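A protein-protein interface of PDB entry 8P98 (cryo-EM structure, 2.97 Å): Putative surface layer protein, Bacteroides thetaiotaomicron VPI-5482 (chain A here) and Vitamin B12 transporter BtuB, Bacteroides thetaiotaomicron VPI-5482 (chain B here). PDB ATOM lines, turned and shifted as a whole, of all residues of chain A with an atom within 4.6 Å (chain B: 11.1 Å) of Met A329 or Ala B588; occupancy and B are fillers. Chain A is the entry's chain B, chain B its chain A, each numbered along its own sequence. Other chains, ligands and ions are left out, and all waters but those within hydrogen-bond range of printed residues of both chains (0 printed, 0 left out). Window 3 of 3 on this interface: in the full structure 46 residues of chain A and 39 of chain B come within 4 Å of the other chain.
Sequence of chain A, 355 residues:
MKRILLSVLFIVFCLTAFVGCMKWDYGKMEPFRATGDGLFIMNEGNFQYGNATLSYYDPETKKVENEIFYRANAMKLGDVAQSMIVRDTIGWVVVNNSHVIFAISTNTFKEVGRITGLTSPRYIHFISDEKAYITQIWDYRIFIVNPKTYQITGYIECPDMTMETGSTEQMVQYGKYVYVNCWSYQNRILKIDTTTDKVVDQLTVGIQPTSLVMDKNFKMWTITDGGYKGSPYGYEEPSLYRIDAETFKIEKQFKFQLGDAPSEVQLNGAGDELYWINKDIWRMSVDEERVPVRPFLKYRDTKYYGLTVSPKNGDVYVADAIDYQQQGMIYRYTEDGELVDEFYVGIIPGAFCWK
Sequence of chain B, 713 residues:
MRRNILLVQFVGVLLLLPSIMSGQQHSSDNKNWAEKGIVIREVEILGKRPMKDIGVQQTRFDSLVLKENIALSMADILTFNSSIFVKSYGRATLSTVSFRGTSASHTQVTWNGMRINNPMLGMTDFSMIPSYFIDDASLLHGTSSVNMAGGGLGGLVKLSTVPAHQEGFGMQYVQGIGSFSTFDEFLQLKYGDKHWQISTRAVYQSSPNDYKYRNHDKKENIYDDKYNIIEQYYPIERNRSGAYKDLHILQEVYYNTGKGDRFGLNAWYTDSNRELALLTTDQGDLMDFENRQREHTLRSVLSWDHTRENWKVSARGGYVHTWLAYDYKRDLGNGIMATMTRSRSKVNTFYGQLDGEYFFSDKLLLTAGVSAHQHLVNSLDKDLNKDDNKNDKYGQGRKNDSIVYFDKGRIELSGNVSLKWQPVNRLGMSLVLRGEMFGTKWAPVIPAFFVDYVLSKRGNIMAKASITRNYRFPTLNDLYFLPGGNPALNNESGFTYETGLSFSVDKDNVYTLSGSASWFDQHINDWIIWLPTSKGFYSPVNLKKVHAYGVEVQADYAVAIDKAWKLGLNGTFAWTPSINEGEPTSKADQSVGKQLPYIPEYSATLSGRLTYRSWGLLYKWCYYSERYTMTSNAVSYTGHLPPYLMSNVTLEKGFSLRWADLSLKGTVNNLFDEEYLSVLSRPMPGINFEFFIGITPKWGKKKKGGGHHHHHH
The side-chain amide oxygen (OE1) of Gln A326 sits close to the side-chain carboxylate (OD1) of Asp B589, at 3.0 Å. The side-chain hydroxyl (OH) of Tyr A344 sits at hydrogen-bond distance from the side-chain amide nitrogen (NE2) of Gln B590, at 2.5 Å. The side-chain hydroxyl of Thr B631 is in hydrogen-bond range of the side-chain amide nitrogen of Gln A326 (2.9 Å).
OD2 of Asp B589 is in hydrogen-bond range of N of Thr B585, 3.2 Å away. N of Ser B586 lies within hydrogen-bond range of OD2 of Asp B589 (2.7 Å). The side-chain hydroxyl (OG) of Ser B632 lies close to the backbone NH (N) of Ala B634, at 3.4 Å. The backbone NH of Tyr A331 is in hydrogen-bond range of the backbone carbonyl oxygen of Val A318, 3.1 Å away. OD1 of Asp A320 lies within hydrogen-bond range of N of Ile A322. The backbone NH (N) of Asp A320 is in hydrogen-bond range of the backbone carbonyl oxygen (O) of Met A329 (2.8 Å).
Among the printed residues, merely in contact across the chains: Ile A322 with Asp B589 (3.3 Å), Gln A326 with Gln B590 (3.9 Å), Gln A326 with Ser B632 (3.5 Å), Met A329 with Ala B588 (3.6 Å), Tyr A331 with Lys B587 (3.8 Å) and Tyr A344 with Ala B588 (3.6 Å).
Met A329 touches just one residue of chain B: Ala B588. Ala B588 touches two residues of chain A. No residue of chain B comes within 4 Å of Asp A320. No residue of chain B comes within 4 Å of Gly A328. No residue of chain B comes within 4 Å of Ile A330. Tyr A331 touches one residue of chain B. No residue of chain B comes within 4 Å of Phe A343. Tyr A344 touches two residues of chain B. Of the printed residues of chain A, Gln B590 touches Gln A326 and Tyr A344. Printed residues of chain A within 4 Å of Lys B587: Tyr A331 (3.8 Å). Val B592 touches none of the printed residues of chain A. Val A318 touches none of the printed residues of chain B. The nearest residue of chain A that does not touch Ala B588 is Gln A326 (4.4 Å).
Of the 12 printed residues of chain A, 5 touch a printed residue of chain B. Along chain A the printed residues that touch a printed residue of chain B span positions 322 to 344. Of the 16 printed residues of chain B, 6 touch a printed residue of chain A. Hydrophobic or aromatic side chains of chain B that line the printed part of chain A: Ala B588. Among the printed residues, 9 pairs touch across the chains.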
ATOM      1  N   VAL A 318      16.703  14.476  29.872  1.00  0.00           N
ATOM      2  CA  VAL A 318      15.588  14.890  29.032  1.00  0.00           C
ATOM      3  C   VAL A 318      16.046  16.061  28.179  1.00  0.00           C
ATOM      4  O   VAL A 318      16.446  17.101  28.710  1.00  0.00           O
ATOM      5  CB  VAL A 318      14.357  15.272  29.869  1.00  0.00           C
ATOM      6  CG1 VAL A 318      13.246  15.769  28.968  1.00  0.00           C
ATOM      7  CG2 VAL A 318      13.894  14.088  30.693  1.00  0.00           C
ATOM      8  N   ALA A 319      15.981  15.893  26.861  1.00  0.00           N
ATOM      9  CA  ALA A 319      16.428  16.909  25.922  1.00  0.00           C
ATOM     10  C   ALA A 319      15.291  17.875  25.633  1.00  0.00           C
ATOM     11  O   ALA A 319      14.207  17.458  25.215  1.00  0.00           O
ATOM     12  CB  ALA A 319      16.921  16.275  24.623  1.00  0.00           C
ATOM     13  N   ASP A 320      15.544  19.161  25.850  1.00  0.00           N
ATOM     14  CA  ASP A 320      14.559  20.210  25.629  1.00  0.00           C
ATOM     15  C   ASP A 320      14.927  20.964  24.363  1.00  0.00           C
ATOM     16  O   ASP A 320      16.073  21.400  24.209  1.00  0.00           O
ATOM     17  CB  ASP A 320      14.498  21.159  26.826  1.00  0.00           C
ATOM     18  CG  ASP A 320      13.194  21.925  26.899  1.00  0.00           C
ATOM     19  OD1 ASP A 320      12.762  22.473  25.864  1.00  0.00           O
ATOM     20  OD2 ASP A 320      12.603  21.987  27.995  1.00  0.00           O
ATOM     21  N   ILE A 322      13.292  23.761  23.474  1.00  0.00           N
ATOM     22  CA  ILE A 322      12.953  25.157  23.735  1.00  0.00           C
ATOM     23  C   ILE A 322      12.027  25.674  22.639  1.00  0.00           C
ATOM     24  O   ILE A 322      10.836  25.342  22.614  1.00  0.00           O
ATOM     25  CB  ILE A 322      14.219  26.026  23.862  1.00  0.00           C
ATOM     26  CG1 ILE A 322      15.211  25.371  24.816  1.00  0.00           C
ATOM     27  CG2 ILE A 322      13.877  27.399  24.408  1.00  0.00           C
ATOM     28  CD1 ILE A 322      14.673  25.198  26.214  1.00  0.00           C
ATOM     29  N   GLN A 326      17.278  28.319  19.138  1.00  0.00           N
ATOM     30  CA  GLN A 326      18.391  28.650  20.016  1.00  0.00           C
ATOM     31  C   GLN A 326      18.825  27.381  20.736  1.00  0.00           C
ATOM     32  O   GLN A 326      18.214  26.319  20.587  1.00  0.00           O
ATOM     33  CB  GLN A 326      18.012  29.755  21.004  1.00  0.00           C
ATOM     34  CG  GLN A 326      16.933  29.355  21.985  1.00  0.00           C
ATOM     35  CD  GLN A 326      16.540  30.486  22.904  1.00  0.00           C
ATOM     36  OE1 GLN A 326      15.638  30.343  23.728  1.00  0.00           O
ATOM     37  NE2 GLN A 326      17.219  31.616  22.774  1.00  0.00           N
ATOM     38  N   GLN A 327      19.889  27.502  21.522  1.00  0.00           N
ATOM     39  CA  GLN A 327      20.468  26.348  22.193  1.00  0.00           C
ATOM     40  C   GLN A 327      19.468  25.721  23.155  1.00  0.00           C
ATOM     41  O   GLN A 327      18.852  26.413  23.969  1.00  0.00           O
ATOM     42  CB  GLN A 327      21.729  26.767  22.945  1.00  0.00           C
ATOM     43  CG  GLN A 327      22.917  27.069  22.051  1.00  0.00           C
ATOM     44  CD  GLN A 327      24.231  27.014  22.799  1.00  0.00           C
ATOM     45  OE1 GLN A 327      24.364  27.576  23.884  1.00  0.00           O
ATOM     46  NE2 GLN A 327      25.209  26.331  22.224  1.00  0.00           N
ATOM     47  N   GLY A 328      19.314  24.403  23.062  1.00  0.00           N
ATOM     48  CA  GLY A 328      18.480  23.673  23.990  1.00  0.00           C
ATOM     49  C   GLY A 328      19.228  23.304  25.255  1.00  0.00           C
ATOM     50  O   GLY A 328      20.402  23.623  25.440  1.00  0.00           O
ATOM     51  N   MET A 329      18.525  22.613  26.147  1.00  0.00           N
ATOM     52  CA  MET A 329      19.120  22.159  27.394  1.00  0.00           C
ATOM     53  C   MET A 329      18.712  20.726  27.676  1.00  0.00           C
ATOM     54  O   MET A 329      17.650  20.276  27.241  1.00  0.00           O
ATOM     55  CB  MET A 329      18.705  23.033  28.580  1.00  0.00           C
ATOM     56  CG  MET A 329      19.227  24.448  28.533  1.00  0.00           C
ATOM     57  SD  MET A 329      18.751  25.389  29.990  1.00  0.00           S
ATOM     58  CE  MET A 329      17.020  25.662  29.644  1.00  0.00           C
ATOM     59  N   ILE A 330      19.563  20.019  28.411  1.00  0.00           N
ATOM     60  CA  ILE A 330      19.236  18.713  28.966  1.00  0.00           C
ATOM     61  C   ILE A 330      19.116  18.852  30.473  1.00  0.00           C
ATOM     62  O   ILE A 330      20.008  19.403  31.128  1.00  0.00           O
ATOM     63  CB  ILE A 330      20.284  17.651  28.594  1.00  0.00           C
ATOM     64  CG1 ILE A 330      20.311  17.412  27.087  1.00  0.00           C
ATOM     65  CG2 ILE A 330      20.014  16.355  29.332  1.00  0.00           C
ATOM     66  CD1 ILE A 330      21.245  18.297  26.349  1.00  0.00           C
ATOM     67  N   TYR A 331      18.011  18.365  31.020  1.00  0.00           N
ATOM     68  CA  TYR A 331      17.778  18.378  32.454  1.00  0.00           C
ATOM     69  C   TYR A 331      18.120  17.000  32.998  1.00  0.00           C
ATOM     70  O   TYR A 331      17.547  15.998  32.561  1.00  0.00           O
ATOM     71  CB  TYR A 331      16.329  18.744  32.763  1.00  0.00           C
ATOM     72  CG  TYR A 331      15.903  20.059  32.160  1.00  0.00           C
ATOM     73  CD1 TYR A 331      16.511  21.247  32.534  1.00  0.00           C
ATOM     74  CD2 TYR A 331      14.896  20.110  31.210  1.00  0.00           C
ATOM     75  CE1 TYR A 331      16.128  22.447  31.982  1.00  0.00           C
ATOM     76  CE2 TYR A 331      14.507  21.304  30.652  1.00  0.00           C
ATOM     77  CZ  TYR A 331      15.125  22.469  31.042  1.00  0.00           C
ATOM     78  OH  TYR A 331      14.734  23.663  30.485  1.00  0.00           O
ATOM     79  N   PHE A 343      22.503  21.734  31.456  1.00  0.00           N
ATOM     80  CA  PHE A 343      23.571  22.235  30.605  1.00  0.00           C
ATOM     81  C   PHE A 343      23.037  22.494  29.204  1.00  0.00           C
ATOM     82  O   PHE A 343      21.975  22.002  28.820  1.00  0.00           O
ATOM     83  CB  PHE A 343      24.758  21.261  30.544  1.00  0.00           C
ATOM     84  CG  PHE A 343      24.366  19.836  30.269  1.00  0.00           C
ATOM     85  CD1 PHE A 343      23.822  19.043  31.267  1.00  0.00           C
ATOM     86  CD2 PHE A 343      24.538  19.288  29.014  1.00  0.00           C
ATOM     87  CE1 PHE A 343      23.459  17.735  31.017  1.00  0.00           C
ATOM     88  CE2 PHE A 343      24.176  17.977  28.759  1.00  0.00           C
ATOM     89  CZ  PHE A 343      23.636  17.202  29.764  1.00  0.00           C
ATOM     90  N   TYR A 344      23.793  23.279  28.444  1.00  0.00           N
ATOM     91  CA  TYR A 344      23.374  23.763  27.135  1.00  0.00           C
ATOM     92  C   TYR A 344      24.076  22.987  26.028  1.00  0.00           C
ATOM     93  O   TYR A 344      25.236  22.592  26.173  1.00  0.00           O
ATOM     94  CB  TYR A 344      23.675  25.256  26.998  1.00  0.00           C
ATOM     95  CG  TYR A 344      22.519  26.153  27.368  1.00  0.00           C
ATOM     96  CD1 TYR A 344      21.451  26.334  26.502  1.00  0.00           C
ATOM     97  CD2 TYR A 344      22.490  26.811  28.587  1.00  0.00           C
ATOM     98  CE1 TYR A 344      20.393  27.155  26.834  1.00  0.00           C
ATOM     99  CE2 TYR A 344      21.433  27.630  28.929  1.00  0.00           C
ATOM    100  CZ  TYR A 344      20.388  27.796  28.051  1.00  0.00           C
ATOM    101  OH  TYR A 344      19.335  28.612  28.388  1.00  0.00           O
ATOM    102  N   ASN B 580      14.936  42.631  21.104  1.00  0.00           N
ATOM    103  CA  ASN B 580      13.717  41.920  21.480  1.00  0.00           C
ATOM    104  C   ASN B 580      13.399  42.254  22.932  1.00  0.00           C
ATOM    105  O   ASN B 580      14.056  41.763  23.852  1.00  0.00           O
ATOM    106  CB  ASN B 580      13.895  40.421  21.278  1.00  0.00           C
ATOM    107  CG  ASN B 580      12.730  39.616  21.815  1.00  0.00           C
ATOM    108  OD1 ASN B 580      11.639  40.140  22.027  1.00  0.00           O
ATOM    109  ND2 ASN B 580      12.961  38.331  22.043  1.00  0.00           N
ATOM    110  N   GLY B 582      10.560  41.493  24.442  1.00  0.00           N
ATOM    111  CA  GLY B 582       9.488  40.662  24.943  1.00  0.00           C
ATOM    112  C   GLY B 582       9.859  39.921  26.211  1.00  0.00           C
ATOM    113  O   GLY B 582      11.027  39.743  26.553  1.00  0.00           O
ATOM    114  N   GLU B 583       8.826  39.494  26.924  1.00  0.00           N
ATOM    115  CA  GLU B 583       9.027  38.684  28.114  1.00  0.00           C
ATOM    116  C   GLU B 583       9.646  37.344  27.725  1.00  0.00           C
ATOM    117  O   GLU B 583       9.331  36.804  26.658  1.00  0.00           O
ATOM    118  CB  GLU B 583       7.693  38.461  28.831  1.00  0.00           C
ATOM    119  CG  GLU B 583       7.787  37.672  30.123  1.00  0.00           C
ATOM    120  CD  GLU B 583       6.437  37.463  30.778  1.00  0.00           C
ATOM    121  OE1 GLU B 583       5.423  37.916  30.209  1.00  0.00           O
ATOM    122  OE2 GLU B 583       6.389  36.841  31.860  1.00  0.00           O
ATOM    123  N   PRO B 584      10.549  36.794  28.544  1.00  0.00           N
ATOM    124  CA  PRO B 584      11.069  35.449  28.268  1.00  0.00           C
ATOM    125  C   PRO B 584       9.954  34.431  28.094  1.00  0.00           C
ATOM    126  O   PRO B 584       9.094  34.293  28.969  1.00  0.00           O
ATOM    127  CB  PRO B 584      11.914  35.142  29.508  1.00  0.00           C
ATOM    128  CG  PRO B 584      12.360  36.469  29.987  1.00  0.00           C
ATOM    129  CD  PRO B 584      11.255  37.441  29.663  1.00  0.00           C
ATOM    130  N   THR B 585       9.959  33.721  26.965  1.00  0.00           N
ATOM    131  CA  THR B 585       8.914  32.735  26.713  1.00  0.00           C
ATOM    132  C   THR B 585       8.954  31.617  27.746  1.00  0.00           C
ATOM    133  O   THR B 585       7.908  31.168  28.229  1.00  0.00           O
ATOM    134  CB  THR B 585       9.058  32.164  25.303  1.00  0.00           C
ATOM    135  OG1 THR B 585      10.319  31.495  25.184  1.00  0.00           O
ATOM    136  CG2 THR B 585       8.985  33.277  24.273  1.00  0.00           C
ATOM    137  N   SER B 586      10.147  31.157  28.096  1.00  0.00           N
ATOM    138  CA  SER B 586      10.333  30.112  29.090  1.00  0.00           C
ATOM    139  C   SER B 586      11.212  30.631  30.224  1.00  0.00           C
ATOM    140  O   SER B 586      11.534  31.820  30.300  1.00  0.00           O
ATOM    141  CB  SER B 586      10.930  28.856  28.453  1.00  0.00           C
ATOM    142  OG  SER B 586      11.172  27.868  29.438  1.00  0.00           O
ATOM    143  N   LYS B 587      11.597  29.718  31.115  1.00  0.00           N
ATOM    144  CA  LYS B 587      12.410  30.094  32.266  1.00  0.00           C
ATOM    145  C   LYS B 587      13.792  30.569  31.836  1.00  0.00           C
ATOM    146  O   LYS B 587      14.350  31.496  32.435  1.00  0.00           O
ATOM    147  CB  LYS B 587      12.522  28.911  33.226  1.00  0.00           C
ATOM    148  CG  LYS B 587      13.345  27.756  32.679  1.00  0.00           C
ATOM    149  CD  LYS B 587      13.335  26.571  33.605  1.00  0.00           C
ATOM    150  CE  LYS B 587      11.995  25.888  33.513  1.00  0.00           C
ATOM    151  NZ  LYS B 587      11.784  25.373  32.130  1.00  0.00           N
ATOM    152  N   ALA B 588      14.358  29.952  30.799  1.00  0.00           N
ATOM    153  CA  ALA B 588      15.733  30.206  30.375  1.00  0.00           C
ATOM    154  C   ALA B 588      15.736  30.439  28.870  1.00  0.00           C
ATOM    155  O   ALA B 588      15.847  29.496  28.083  1.00  0.00           O
ATOM    156  CB  ALA B 588      16.647  29.053  30.769  1.00  0.00           C
ATOM    157  N   ASP B 589      15.607  31.703  28.478  1.00  0.00           N
ATOM    158  CA  ASP B 589      15.738  32.121  27.088  1.00  0.00           C
ATOM    159  C   ASP B 589      16.725  33.276  27.054  1.00  0.00           C
ATOM    160  O   ASP B 589      16.482  34.321  27.663  1.00  0.00           O
ATOM    161  CB  ASP B 589      14.391  32.536  26.500  1.00  0.00           C
ATOM    162  CG  ASP B 589      13.444  31.369  26.340  1.00  0.00           C
ATOM    163  OD1 ASP B 589      13.927  30.236  26.150  1.00  0.00           O
ATOM    164  OD2 ASP B 589      12.216  31.586  26.400  1.00  0.00           O
ATOM    165  N   GLN B 590      17.837  33.090  26.351  1.00  0.00           N
ATOM    166  CA  GLN B 590      18.822  34.149  26.203  1.00  0.00           C
ATOM    167  C   GLN B 590      18.487  35.100  25.070  1.00  0.00           C
ATOM    168  O   GLN B 590      19.388  35.768  24.558  1.00  0.00           O
ATOM    169  CB  GLN B 590      20.217  33.559  25.987  1.00  0.00           C
ATOM    170  CG  GLN B 590      20.791  32.841  27.193  1.00  0.00           C
ATOM    171  CD  GLN B 590      20.313  31.412  27.300  1.00  0.00           C
ATOM    172  OE1 GLN B 590      19.825  30.834  26.330  1.00  0.00           O
ATOM    173  NE2 GLN B 590      20.446  30.832  28.485  1.00  0.00           N
ATOM    174  N   SER B 591      17.221  35.167  24.660  1.00  0.00           N
ATOM    175  CA  SER B 591      16.819  36.008  23.543  1.00  0.00           C
ATOM    176  C   SER B 591      16.425  37.418  23.956  1.00  0.00           C
ATOM    177  O   SER B 591      16.402  38.312  23.104  1.00  0.00           O
ATOM    178  CB  SER B 591      15.650  35.361  22.798  1.00  0.00           C
ATOM    179  OG  SER B 591      14.496  35.313  23.615  1.00  0.00           O
ATOM    180  N   VAL B 592      16.123  37.639  25.227  1.00  0.00           N
ATOM    181  CA  VAL B 592      15.652  38.940  25.685  1.00  0.00           C
ATOM    182  C   VAL B 592      16.797  39.940  25.655  1.00  0.00           C
ATOM    183  O   VAL B 592      17.919  39.638  26.076  1.00  0.00           O
ATOM    184  CB  VAL B 592      15.045  38.824  27.091  1.00  0.00           C
ATOM    185  CG1 VAL B 592      14.410  40.139  27.502  1.00  0.00           C
ATOM    186  CG2 VAL B 592      14.027  37.707  27.119  1.00  0.00           C
ATOM    187  N   LYS B 594      18.355  41.010  23.092  1.00  0.00           N
ATOM    188  CA  LYS B 594      19.337  40.631  22.090  1.00  0.00           C
ATOM    189  C   LYS B 594      18.897  41.080  20.704  1.00  0.00           C
ATOM    190  O   LYS B 594      17.723  41.364  20.460  1.00  0.00           O
ATOM    191  CB  LYS B 594      19.554  39.116  22.092  1.00  0.00           C
ATOM    192  CG  LYS B 594      19.924  38.541  23.441  1.00  0.00           C
ATOM    193  CD  LYS B 594      21.248  39.076  23.947  1.00  0.00           C
ATOM    194  CE  LYS B 594      21.705  38.307  25.173  1.00  0.00           C
ATOM    195  NZ  LYS B 594      23.034  38.769  25.650  1.00  0.00           N
ATOM    196  N   THR B 631      18.589  33.288  17.978  1.00  0.00           N
ATOM    197  CA  THR B 631      17.930  34.312  18.781  1.00  0.00           C
ATOM    198  C   THR B 631      18.783  34.697  19.982  1.00  0.00           C
ATOM    199  O   THR B 631      18.878  35.878  20.335  1.00  0.00           O
ATOM    200  CB  THR B 631      16.559  33.820  19.241  1.00  0.00           C
ATOM    201  OG1 THR B 631      16.724  32.704  20.123  1.00  0.00           O
ATOM    202  CG2 THR B 631      15.721  33.394  18.051  1.00  0.00           C
ATOM    203  N   SER B 632      19.418  33.713  20.618  1.00  0.00           N
ATOM    204  CA  SER B 632      20.208  33.957  21.816  1.00  0.00           C
ATOM    205  C   SER B 632      21.473  34.755  21.546  1.00  0.00           C
ATOM    206  O   SER B 632      22.113  35.198  22.504  1.00  0.00           O
ATOM    207  CB  SER B 632      20.579  32.628  22.472  1.00  0.00           C
ATOM    208  OG  SER B 632      21.330  31.818  21.586  1.00  0.00           O
ATOM    209  N   ALA B 634      24.152  33.538  20.732  1.00  0.00           N
ATOM    210  CA  ALA B 634      25.212  32.742  21.326  1.00  0.00           C
ATOM    211  C   ALA B 634      26.387  32.616  20.366  1.00  0.00           C
ATOM    212  O   ALA B 634      26.221  32.585  19.145  1.00  0.00           O
ATOM    213  CB  ALA B 634      24.692  31.355  21.699  1.00  0.00           C
